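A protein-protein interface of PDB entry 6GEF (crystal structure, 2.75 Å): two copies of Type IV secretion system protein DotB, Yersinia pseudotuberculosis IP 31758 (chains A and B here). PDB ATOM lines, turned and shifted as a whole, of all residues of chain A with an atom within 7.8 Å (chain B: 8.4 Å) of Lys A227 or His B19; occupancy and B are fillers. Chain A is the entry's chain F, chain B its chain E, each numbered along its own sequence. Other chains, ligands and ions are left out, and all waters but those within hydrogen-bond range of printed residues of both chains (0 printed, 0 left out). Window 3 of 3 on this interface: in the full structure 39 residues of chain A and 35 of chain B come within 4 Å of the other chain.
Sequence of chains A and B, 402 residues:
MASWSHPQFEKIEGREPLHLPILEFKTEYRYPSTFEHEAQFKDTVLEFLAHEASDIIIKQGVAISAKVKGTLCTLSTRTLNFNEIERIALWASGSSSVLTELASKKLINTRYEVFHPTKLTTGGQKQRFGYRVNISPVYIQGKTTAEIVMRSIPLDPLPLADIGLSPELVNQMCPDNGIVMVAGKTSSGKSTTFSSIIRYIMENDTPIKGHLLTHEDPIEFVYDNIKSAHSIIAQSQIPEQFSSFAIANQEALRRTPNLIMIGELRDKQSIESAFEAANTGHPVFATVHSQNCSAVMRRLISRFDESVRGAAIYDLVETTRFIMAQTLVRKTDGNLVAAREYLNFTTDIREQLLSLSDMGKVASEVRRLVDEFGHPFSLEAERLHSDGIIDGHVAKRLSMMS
Of the 11 printed residues of chain B, 4 touch a printed residue of chain A. Hydrophobic or aromatic side chains of chain B that line the printed part of chain A: His B19.
OD1 of Asp A224 lies within hydrogen-bond range of N of Gln B141 (3.1 Å).
Of the printed residues of chain B, Asp A224 touches Gln B141. Asn A225 touches none of the printed residues of chain B. Ser A228 touches none of the printed residues of chain B. Printed residues of chain B within 4 Å of Ala A229: Leu B20 (3.5 Å) and Pro B21 (3.2 Å). No residue of chain A comes within 4 Å of Leu B18. Of chain A, only Lys A227 (3.7 Å) comes within 4 Å of His B19. Printed residues of chain A within 4 Å of Leu B20: Ala A229. Of the printed residues of chain A, Pro B21 touches Ala A229 (3.2 Å). Of the printed residues of chain A, Gln B141 touches Asp A224. The nearest residue of chain A that does not touch His B19 is Ala A229 (4.2 Å).
CB of His B19 touches CB of Lys A227, 3.7 Å away. O of Leu B20 touches O of Ala A229, at 3.5 Å. Ala A229 touches Pro B21 (O to CA, 3.2 Å).
The backbone carbonyl oxygen (O) of Asp A224 sits at hydrogen-bond distance from the side-chain amino group (NZ) of Lys A227 (3.2 Å).
No position is printed for both chains.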
ATOM      1  N   GLY A 123     -15.661  -9.173  10.134  1.00  0.00           N
ATOM      2  CA  GLY A 123     -16.193 -10.258   9.353  1.00  0.00           C
ATOM      3  C   GLY A 123     -15.114 -11.066   8.608  1.00  0.00           C
ATOM      4  O   GLY A 123     -15.049 -11.075   7.374  1.00  0.00           O
ATOM      5  N   GLN A 125     -11.174 -13.449   9.150  1.00  0.00           N
ATOM      6  CA  GLN A 125     -10.156 -14.340   9.647  1.00  0.00           C
ATOM      7  C   GLN A 125      -9.009 -13.541  10.255  1.00  0.00           C
ATOM      8  O   GLN A 125      -9.171 -12.355  10.560  1.00  0.00           O
ATOM      9  CB  GLN A 125      -9.693 -15.274   8.505  1.00  0.00           C
ATOM     10  CG  GLN A 125      -9.355 -14.559   7.206  1.00  0.00           C
ATOM     11  CD  GLN A 125     -10.565 -13.910   6.557  1.00  0.00           C
ATOM     12  OE1 GLN A 125     -11.286 -14.555   5.824  1.00  0.00           O
ATOM     13  NE2 GLN A 125     -10.789 -12.635   6.838  1.00  0.00           N
ATOM     14  N   ARG A 199     -10.268  -2.125  -7.187  1.00  0.00           N
ATOM     15  CA  ARG A 199     -11.295  -2.326  -6.169  1.00  0.00           C
ATOM     16  C   ARG A 199     -12.608  -1.689  -6.585  1.00  0.00           C
ATOM     17  O   ARG A 199     -13.665  -2.313  -6.478  1.00  0.00           O
ATOM     18  CB  ARG A 199     -10.800  -1.782  -4.816  1.00  0.00           C
ATOM     19  CG  ARG A 199     -11.829  -1.858  -3.709  1.00  0.00           C
ATOM     20  CD  ARG A 199     -11.619  -0.785  -2.696  1.00  0.00           C
ATOM     21  NE  ARG A 199     -12.662  -0.759  -1.668  1.00  0.00           N
ATOM     22  CZ  ARG A 199     -12.433  -0.733  -0.368  1.00  0.00           C
ATOM     23  NH1 ARG A 199     -11.184  -0.703   0.086  1.00  0.00           N
ATOM     24  NH2 ARG A 199     -13.453  -0.713   0.479  1.00  0.00           N
ATOM     25  N   MET A 202     -14.241  -3.787  -9.243  1.00  0.00           N
ATOM     26  CA  MET A 202     -14.886  -4.991  -8.687  1.00  0.00           C
ATOM     27  C   MET A 202     -16.171  -4.680  -7.932  1.00  0.00           C
ATOM     28  O   MET A 202     -17.146  -5.404  -8.070  1.00  0.00           O
ATOM     29  CB  MET A 202     -13.908  -5.736  -7.777  1.00  0.00           C
ATOM     30  CG  MET A 202     -12.755  -6.396  -8.476  1.00  0.00           C
ATOM     31  SD  MET A 202     -11.729  -7.331  -7.324  1.00  0.00           S
ATOM     32  CE  MET A 202     -11.107  -6.032  -6.302  1.00  0.00           C
ATOM     33  N   GLU A 203     -16.178  -3.571  -7.226  1.00  0.00           N
ATOM     34  CA  GLU A 203     -17.261  -3.258  -6.293  1.00  0.00           C
ATOM     35  C   GLU A 203     -18.446  -2.586  -6.948  1.00  0.00           C
ATOM     36  O   GLU A 203     -19.535  -2.583  -6.374  1.00  0.00           O
ATOM     37  CB  GLU A 203     -16.747  -2.392  -5.119  1.00  0.00           C
ATOM     38  CG  GLU A 203     -15.705  -3.083  -4.246  1.00  0.00           C
ATOM     39  CD  GLU A 203     -15.530  -2.477  -2.905  1.00  0.00           C
ATOM     40  OE1 GLU A 203     -15.661  -3.210  -1.878  1.00  0.00           O
ATOM     41  OE2 GLU A 203     -15.307  -1.281  -2.867  1.00  0.00           O
ATOM     42  N   ASN A 204     -18.259  -2.015  -8.135  1.00  0.00           N
ATOM     43  CA  ASN A 204     -19.281  -1.222  -8.811  1.00  0.00           C
ATOM     44  C   ASN A 204     -19.561  -1.799 -10.185  1.00  0.00           C
ATOM     45  O   ASN A 204     -18.859  -2.689 -10.679  1.00  0.00           O
ATOM     46  CB  ASN A 204     -18.839   0.240  -8.925  1.00  0.00           C
ATOM     47  CG  ASN A 204     -18.687   0.921  -7.572  1.00  0.00           C
ATOM     48  OD1 ASN A 204     -17.718   0.742  -6.897  1.00  0.00           O
ATOM     49  ND2 ASN A 204     -19.664   1.707  -7.178  1.00  0.00           N
ATOM     50  N   TYR A 223      -6.515  -8.128  -2.752  1.00  0.00           N
ATOM     51  CA  TYR A 223      -7.975  -7.979  -2.869  1.00  0.00           C
ATOM     52  C   TYR A 223      -8.725  -9.140  -2.249  1.00  0.00           C
ATOM     53  O   TYR A 223      -9.798  -9.528  -2.704  1.00  0.00           O
ATOM     54  CB  TYR A 223      -8.375  -7.795  -4.347  1.00  0.00           C
ATOM     55  CG  TYR A 223      -7.565  -6.761  -5.084  1.00  0.00           C
ATOM     56  CD1 TYR A 223      -6.325  -7.055  -5.592  1.00  0.00           C
ATOM     57  CD2 TYR A 223      -8.064  -5.488  -5.272  1.00  0.00           C
ATOM     58  CE1 TYR A 223      -5.574  -6.105  -6.265  1.00  0.00           C
ATOM     59  CE2 TYR A 223      -7.336  -4.512  -5.957  1.00  0.00           C
ATOM     60  CZ  TYR A 223      -6.109  -4.835  -6.458  1.00  0.00           C
ATOM     61  OH  TYR A 223      -5.377  -3.877  -7.127  1.00  0.00           O
ATOM     62  N   ASP A 224      -8.164  -9.708  -1.181  1.00  0.00           N
ATOM     63  CA  ASP A 224      -8.840 -10.822  -0.479  1.00  0.00           C
ATOM     64  C   ASP A 224     -10.072 -10.326   0.240  1.00  0.00           C
ATOM     65  O   ASP A 224     -11.056 -11.080   0.339  1.00  0.00           O
ATOM     66  CB  ASP A 224      -7.872 -11.492   0.468  1.00  0.00           C
ATOM     67  CG  ASP A 224      -6.638 -12.039  -0.257  1.00  0.00           C
ATOM     68  OD1 ASP A 224      -6.754 -13.044  -0.971  1.00  0.00           O
ATOM     69  OD2 ASP A 224      -5.539 -11.505  -0.100  1.00  0.00           O
ATOM     70  N   ASN A 225     -10.069  -9.097   0.729  1.00  0.00           N
ATOM     71  CA  ASN A 225     -11.215  -8.562   1.480  1.00  0.00           C
ATOM     72  C   ASN A 225     -12.139  -7.707   0.606  1.00  0.00           C
ATOM     73  O   ASN A 225     -13.040  -7.081   1.127  1.00  0.00           O
ATOM     74  CB  ASN A 225     -10.723  -7.739   2.680  1.00  0.00           C
ATOM     75  CG  ASN A 225      -9.699  -8.456   3.509  1.00  0.00           C
ATOM     76  OD1 ASN A 225      -8.513  -8.233   3.336  1.00  0.00           O
ATOM     77  ND2 ASN A 225     -10.152  -9.306   4.421  1.00  0.00           N
ATOM     78  N   ILE A 226     -11.938  -7.693  -0.703  1.00  0.00           N
ATOM     79  CA  ILE A 226     -12.777  -6.947  -1.623  1.00  0.00           C
ATOM     80  C   ILE A 226     -13.803  -7.923  -2.210  1.00  0.00           C
ATOM     81  O   ILE A 226     -13.477  -8.828  -2.958  1.00  0.00           O
ATOM     82  CB  ILE A 226     -11.945  -6.308  -2.750  1.00  0.00           C
ATOM     83  CG1 ILE A 226     -10.760  -5.546  -2.175  1.00  0.00           C
ATOM     84  CG2 ILE A 226     -12.838  -5.409  -3.619  1.00  0.00           C
ATOM     85  CD1 ILE A 226     -11.144  -4.401  -1.252  1.00  0.00           C
ATOM     86  N   LYS A 227     -15.058  -7.758  -1.815  1.00  0.00           N
ATOM     87  CA  LYS A 227     -16.154  -8.588  -2.274  1.00  0.00           C
ATOM     88  C   LYS A 227     -16.722  -7.985  -3.549  1.00  0.00           C
ATOM     89  O   LYS A 227     -17.094  -6.811  -3.584  1.00  0.00           O
ATOM     90  CB  LYS A 227     -17.247  -8.671  -1.214  1.00  0.00           C
ATOM     91  CG  LYS A 227     -16.747  -9.143   0.155  1.00  0.00           C
ATOM     92  CD  LYS A 227     -16.323 -10.584   0.017  1.00  0.00           C
ATOM     93  CE  LYS A 227     -15.627 -11.124   1.266  1.00  0.00           C
ATOM     94  NZ  LYS A 227     -14.153 -11.097   1.042  1.00  0.00           N
ATOM     95  N   SER A 228     -16.794  -8.787  -4.613  1.00  0.00           N
ATOM     96  CA  SER A 228     -17.255  -8.359  -5.906  1.00  0.00           C
ATOM     97  C   SER A 228     -18.489  -9.172  -6.305  1.00  0.00           C
ATOM     98  O   SER A 228     -18.639 -10.334  -5.935  1.00  0.00           O
ATOM     99  CB  SER A 228     -16.166  -8.532  -6.963  1.00  0.00           C
ATOM    100  OG  SER A 228     -16.631  -8.108  -8.247  1.00  0.00           O
ATOM    101  N   ALA A 229     -19.368  -8.531  -7.087  1.00  0.00           N
ATOM    102  CA  ALA A 229     -20.573  -9.187  -7.557  1.00  0.00           C
ATOM    103  C   ALA A 229     -20.375  -9.975  -8.850  1.00  0.00           C
ATOM    104  O   ALA A 229     -21.202 -10.798  -9.192  1.00  0.00           O
ATOM    105  CB  ALA A 229     -21.697  -8.153  -7.737  1.00  0.00           C
ATOM    106  N   HIS A 230     -19.307  -9.698  -9.571  1.00  0.00           N
ATOM    107  CA  HIS A 230     -19.255 -10.003 -11.005  1.00  0.00           C
ATOM    108  C   HIS A 230     -17.842 -10.342 -11.462  1.00  0.00           C
ATOM    109  O   HIS A 230     -17.639 -10.751 -12.600  1.00  0.00           O
ATOM    110  CB  HIS A 230     -19.772  -8.802 -11.852  1.00  0.00           C
ATOM    111  CG  HIS A 230     -19.190  -7.489 -11.433  1.00  0.00           C
ATOM    112  ND1 HIS A 230     -17.915  -7.119 -11.751  1.00  0.00           N
ATOM    113  CD2 HIS A 230     -19.712  -6.460 -10.692  1.00  0.00           C
ATOM    114  CE1 HIS A 230     -17.657  -5.923 -11.249  1.00  0.00           C
ATOM    115  NE2 HIS A 230     -18.740  -5.496 -10.610  1.00  0.00           N
ATOM    116  N   SER A 231     -16.862 -10.189 -10.578  1.00  0.00           N
ATOM    117  CA  SER A 231     -15.465 -10.104 -10.948  1.00  0.00           C
ATOM    118  C   SER A 231     -14.649 -11.032 -10.032  1.00  0.00           C
ATOM    119  O   SER A 231     -14.960 -11.185  -8.839  1.00  0.00           O
ATOM    120  CB  SER A 231     -14.948  -8.687 -10.797  1.00  0.00           C
ATOM    121  OG  SER A 231     -15.363  -7.870 -11.881  1.00  0.00           O
ATOM    122  N   PRO B  17     -24.957 -12.059   4.801  1.00  0.00           N
ATOM    123  CA  PRO B  17     -25.410 -12.455   3.420  1.00  0.00           C
ATOM    124  C   PRO B  17     -24.299 -12.138   2.410  1.00  0.00           C
ATOM    125  O   PRO B  17     -24.171 -11.016   1.940  1.00  0.00           O
ATOM    126  CB  PRO B  17     -26.697 -11.719   3.058  1.00  0.00           C
ATOM    127  N   LEU B  18     -23.504 -13.149   2.094  1.00  0.00           N
ATOM    128  CA  LEU B  18     -22.212 -12.943   1.485  1.00  0.00           C
ATOM    129  C   LEU B  18     -22.358 -12.563   0.000  1.00  0.00           C
ATOM    130  O   LEU B  18     -23.333 -12.932  -0.667  1.00  0.00           O
ATOM    131  CB  LEU B  18     -21.362 -14.206   1.630  1.00  0.00           C
ATOM    132  N   HIS B  19     -21.333 -11.883  -0.503  1.00  0.00           N
ATOM    133  CA  HIS B  19     -21.356 -11.384  -1.877  1.00  0.00           C
ATOM    134  C   HIS B  19     -20.790 -12.436  -2.817  1.00  0.00           C
ATOM    135  O   HIS B  19     -19.714 -13.003  -2.523  1.00  0.00           O
ATOM    136  CB  HIS B  19     -20.556 -10.083  -1.985  1.00  0.00           C
ATOM    137  CG  HIS B  19     -21.267  -8.978  -2.681  1.00  0.00           C
ATOM    138  ND1 HIS B  19     -20.672  -7.758  -2.921  1.00  0.00           N
ATOM    139  CD2 HIS B  19     -22.516  -8.893  -3.188  1.00  0.00           C
ATOM    140  CE1 HIS B  19     -21.523  -6.957  -3.543  1.00  0.00           C
ATOM    141  NE2 HIS B  19     -22.655  -7.622  -3.716  1.00  0.00           N
ATOM    142  N   LEU B  20     -21.422 -12.667  -3.931  1.00  0.00           N
ATOM    143  CA  LEU B  20     -21.141 -13.845  -4.764  1.00  0.00           C
ATOM    144  C   LEU B  20     -21.416 -13.429  -6.218  1.00  0.00           C
ATOM    145  O   LEU B  20     -22.373 -12.726  -6.493  1.00  0.00           O
ATOM    146  CB  LEU B  20     -22.026 -15.055  -4.404  1.00  0.00           C
ATOM    147  CG  LEU B  20     -23.511 -14.762  -4.162  1.00  0.00           C
ATOM    148  CD1 LEU B  20     -23.962 -13.430  -4.664  1.00  0.00           C
ATOM    149  CD2 LEU B  20     -24.392 -15.831  -4.746  1.00  0.00           C
ATOM    150  N   PRO B  21     -20.617 -13.916  -7.155  1.00  0.00           N
ATOM    151  CA  PRO B  21     -21.021 -13.932  -8.558  1.00  0.00           C
ATOM    152  C   PRO B  21     -22.356 -14.629  -8.764  1.00  0.00           C
ATOM    153  O   PRO B  21     -22.827 -15.335  -7.906  1.00  0.00           O
ATOM    154  CB  PRO B  21     -19.885 -14.694  -9.266  1.00  0.00           C
ATOM    155  CG  PRO B  21     -18.694 -14.329  -8.466  1.00  0.00           C
ATOM    156  CD  PRO B  21     -19.230 -14.439  -6.999  1.00  0.00           C
ATOM    157  N   ILE B  22     -23.000 -14.343  -9.892  1.00  0.00           N
ATOM    158  CA  ILE B  22     -24.326 -14.847 -10.151  1.00  0.00           C
ATOM    159  C   ILE B  22     -24.310 -16.366 -10.208  1.00  0.00           C
ATOM    160  O   ILE B  22     -23.314 -16.964 -10.610  1.00  0.00           O
ATOM    161  CB  ILE B  22     -24.941 -14.196 -11.379  1.00  0.00           C
ATOM    162  CG1 ILE B  22     -26.448 -14.533 -11.454  1.00  0.00           C
ATOM    163  CG2 ILE B  22     -24.233 -14.607 -12.590  1.00  0.00           C
ATOM    164  CD1 ILE B  22     -27.182 -14.460 -10.104  1.00  0.00           C
ATOM    165  N   GLY B  61     -10.620 -20.037  -2.771  1.00  0.00           N
ATOM    166  CA  GLY B  61     -11.403 -19.033  -2.103  1.00  0.00           C
ATOM    167  C   GLY B  61     -12.520 -18.432  -2.943  1.00  0.00           C
ATOM    168  O   GLY B  61     -13.156 -17.469  -2.503  1.00  0.00           O
ATOM    169  N   VAL B  62     -12.791 -18.975  -4.131  1.00  0.00           N
ATOM    170  CA  VAL B  62     -14.016 -18.688  -4.856  1.00  0.00           C
ATOM    171  C   VAL B  62     -14.564 -19.985  -5.418  1.00  0.00           C
ATOM    172  O   VAL B  62     -13.810 -20.944  -5.658  1.00  0.00           O
ATOM    173  CB  VAL B  62     -13.810 -17.645  -5.989  1.00  0.00           C
ATOM    174  CG1 VAL B  62     -13.174 -16.374  -5.417  1.00  0.00           C
ATOM    175  CG2 VAL B  62     -12.947 -18.240  -7.092  1.00  0.00           C
ATOM    176  N   THR B  77     -22.591 -21.147  -4.234  1.00  0.00           N
ATOM    177  CA  THR B  77     -22.063 -20.040  -3.449  1.00  0.00           C
ATOM    178  C   THR B  77     -20.837 -20.418  -2.623  1.00  0.00           C
ATOM    179  O   THR B  77     -20.231 -19.539  -2.002  1.00  0.00           O
ATOM    180  CB  THR B  77     -23.151 -19.481  -2.514  1.00  0.00           C
ATOM    181  OG1 THR B  77     -22.579 -18.373  -1.804  1.00  0.00           O
ATOM    182  CG2 THR B  77     -23.701 -20.523  -1.556  1.00  0.00           C
ATOM    183  N   THR B  79     -17.087 -21.861  -1.661  1.00  0.00           N
ATOM    184  CA  THR B  79     -15.784 -21.656  -2.248  1.00  0.00           C
ATOM    185  C   THR B  79     -14.976 -22.939  -2.268  1.00  0.00           C
ATOM    186  O   THR B  79     -15.295 -23.921  -1.631  1.00  0.00           O
ATOM    187  CB  THR B  79     -15.038 -20.545  -1.513  1.00  0.00           C
ATOM    188  OG1 THR B  79     -14.639 -21.050  -0.210  1.00  0.00           O
ATOM    189  CG2 THR B  79     -15.896 -19.308  -1.352  1.00  0.00           C
ATOM    190  N   GLN B 141      -4.445 -14.975  -0.143  1.00  0.00           N
ATOM    191  CA  GLN B 141      -4.376 -15.055   1.320  1.00  0.00           C
ATOM    192  C   GLN B 141      -2.957 -15.304   1.791  1.00  0.00           C
ATOM    193  O   GLN B 141      -2.702 -16.158   2.660  1.00  0.00           O
ATOM    194  CB  GLN B 141      -5.352 -16.082   1.880  1.00  0.00           C
ATOM    195  CG  GLN B 141      -6.780 -15.902   1.399  1.00  0.00           C
ATOM    196  CD  GLN B 141      -7.565 -14.797   2.126  1.00  0.00           C
ATOM    197  OE1 GLN B 141      -7.021 -13.782   2.602  1.00  0.00           O
ATOM    198  NE2 GLN B 141      -8.859 -14.973   2.161  1.00  0.00           N
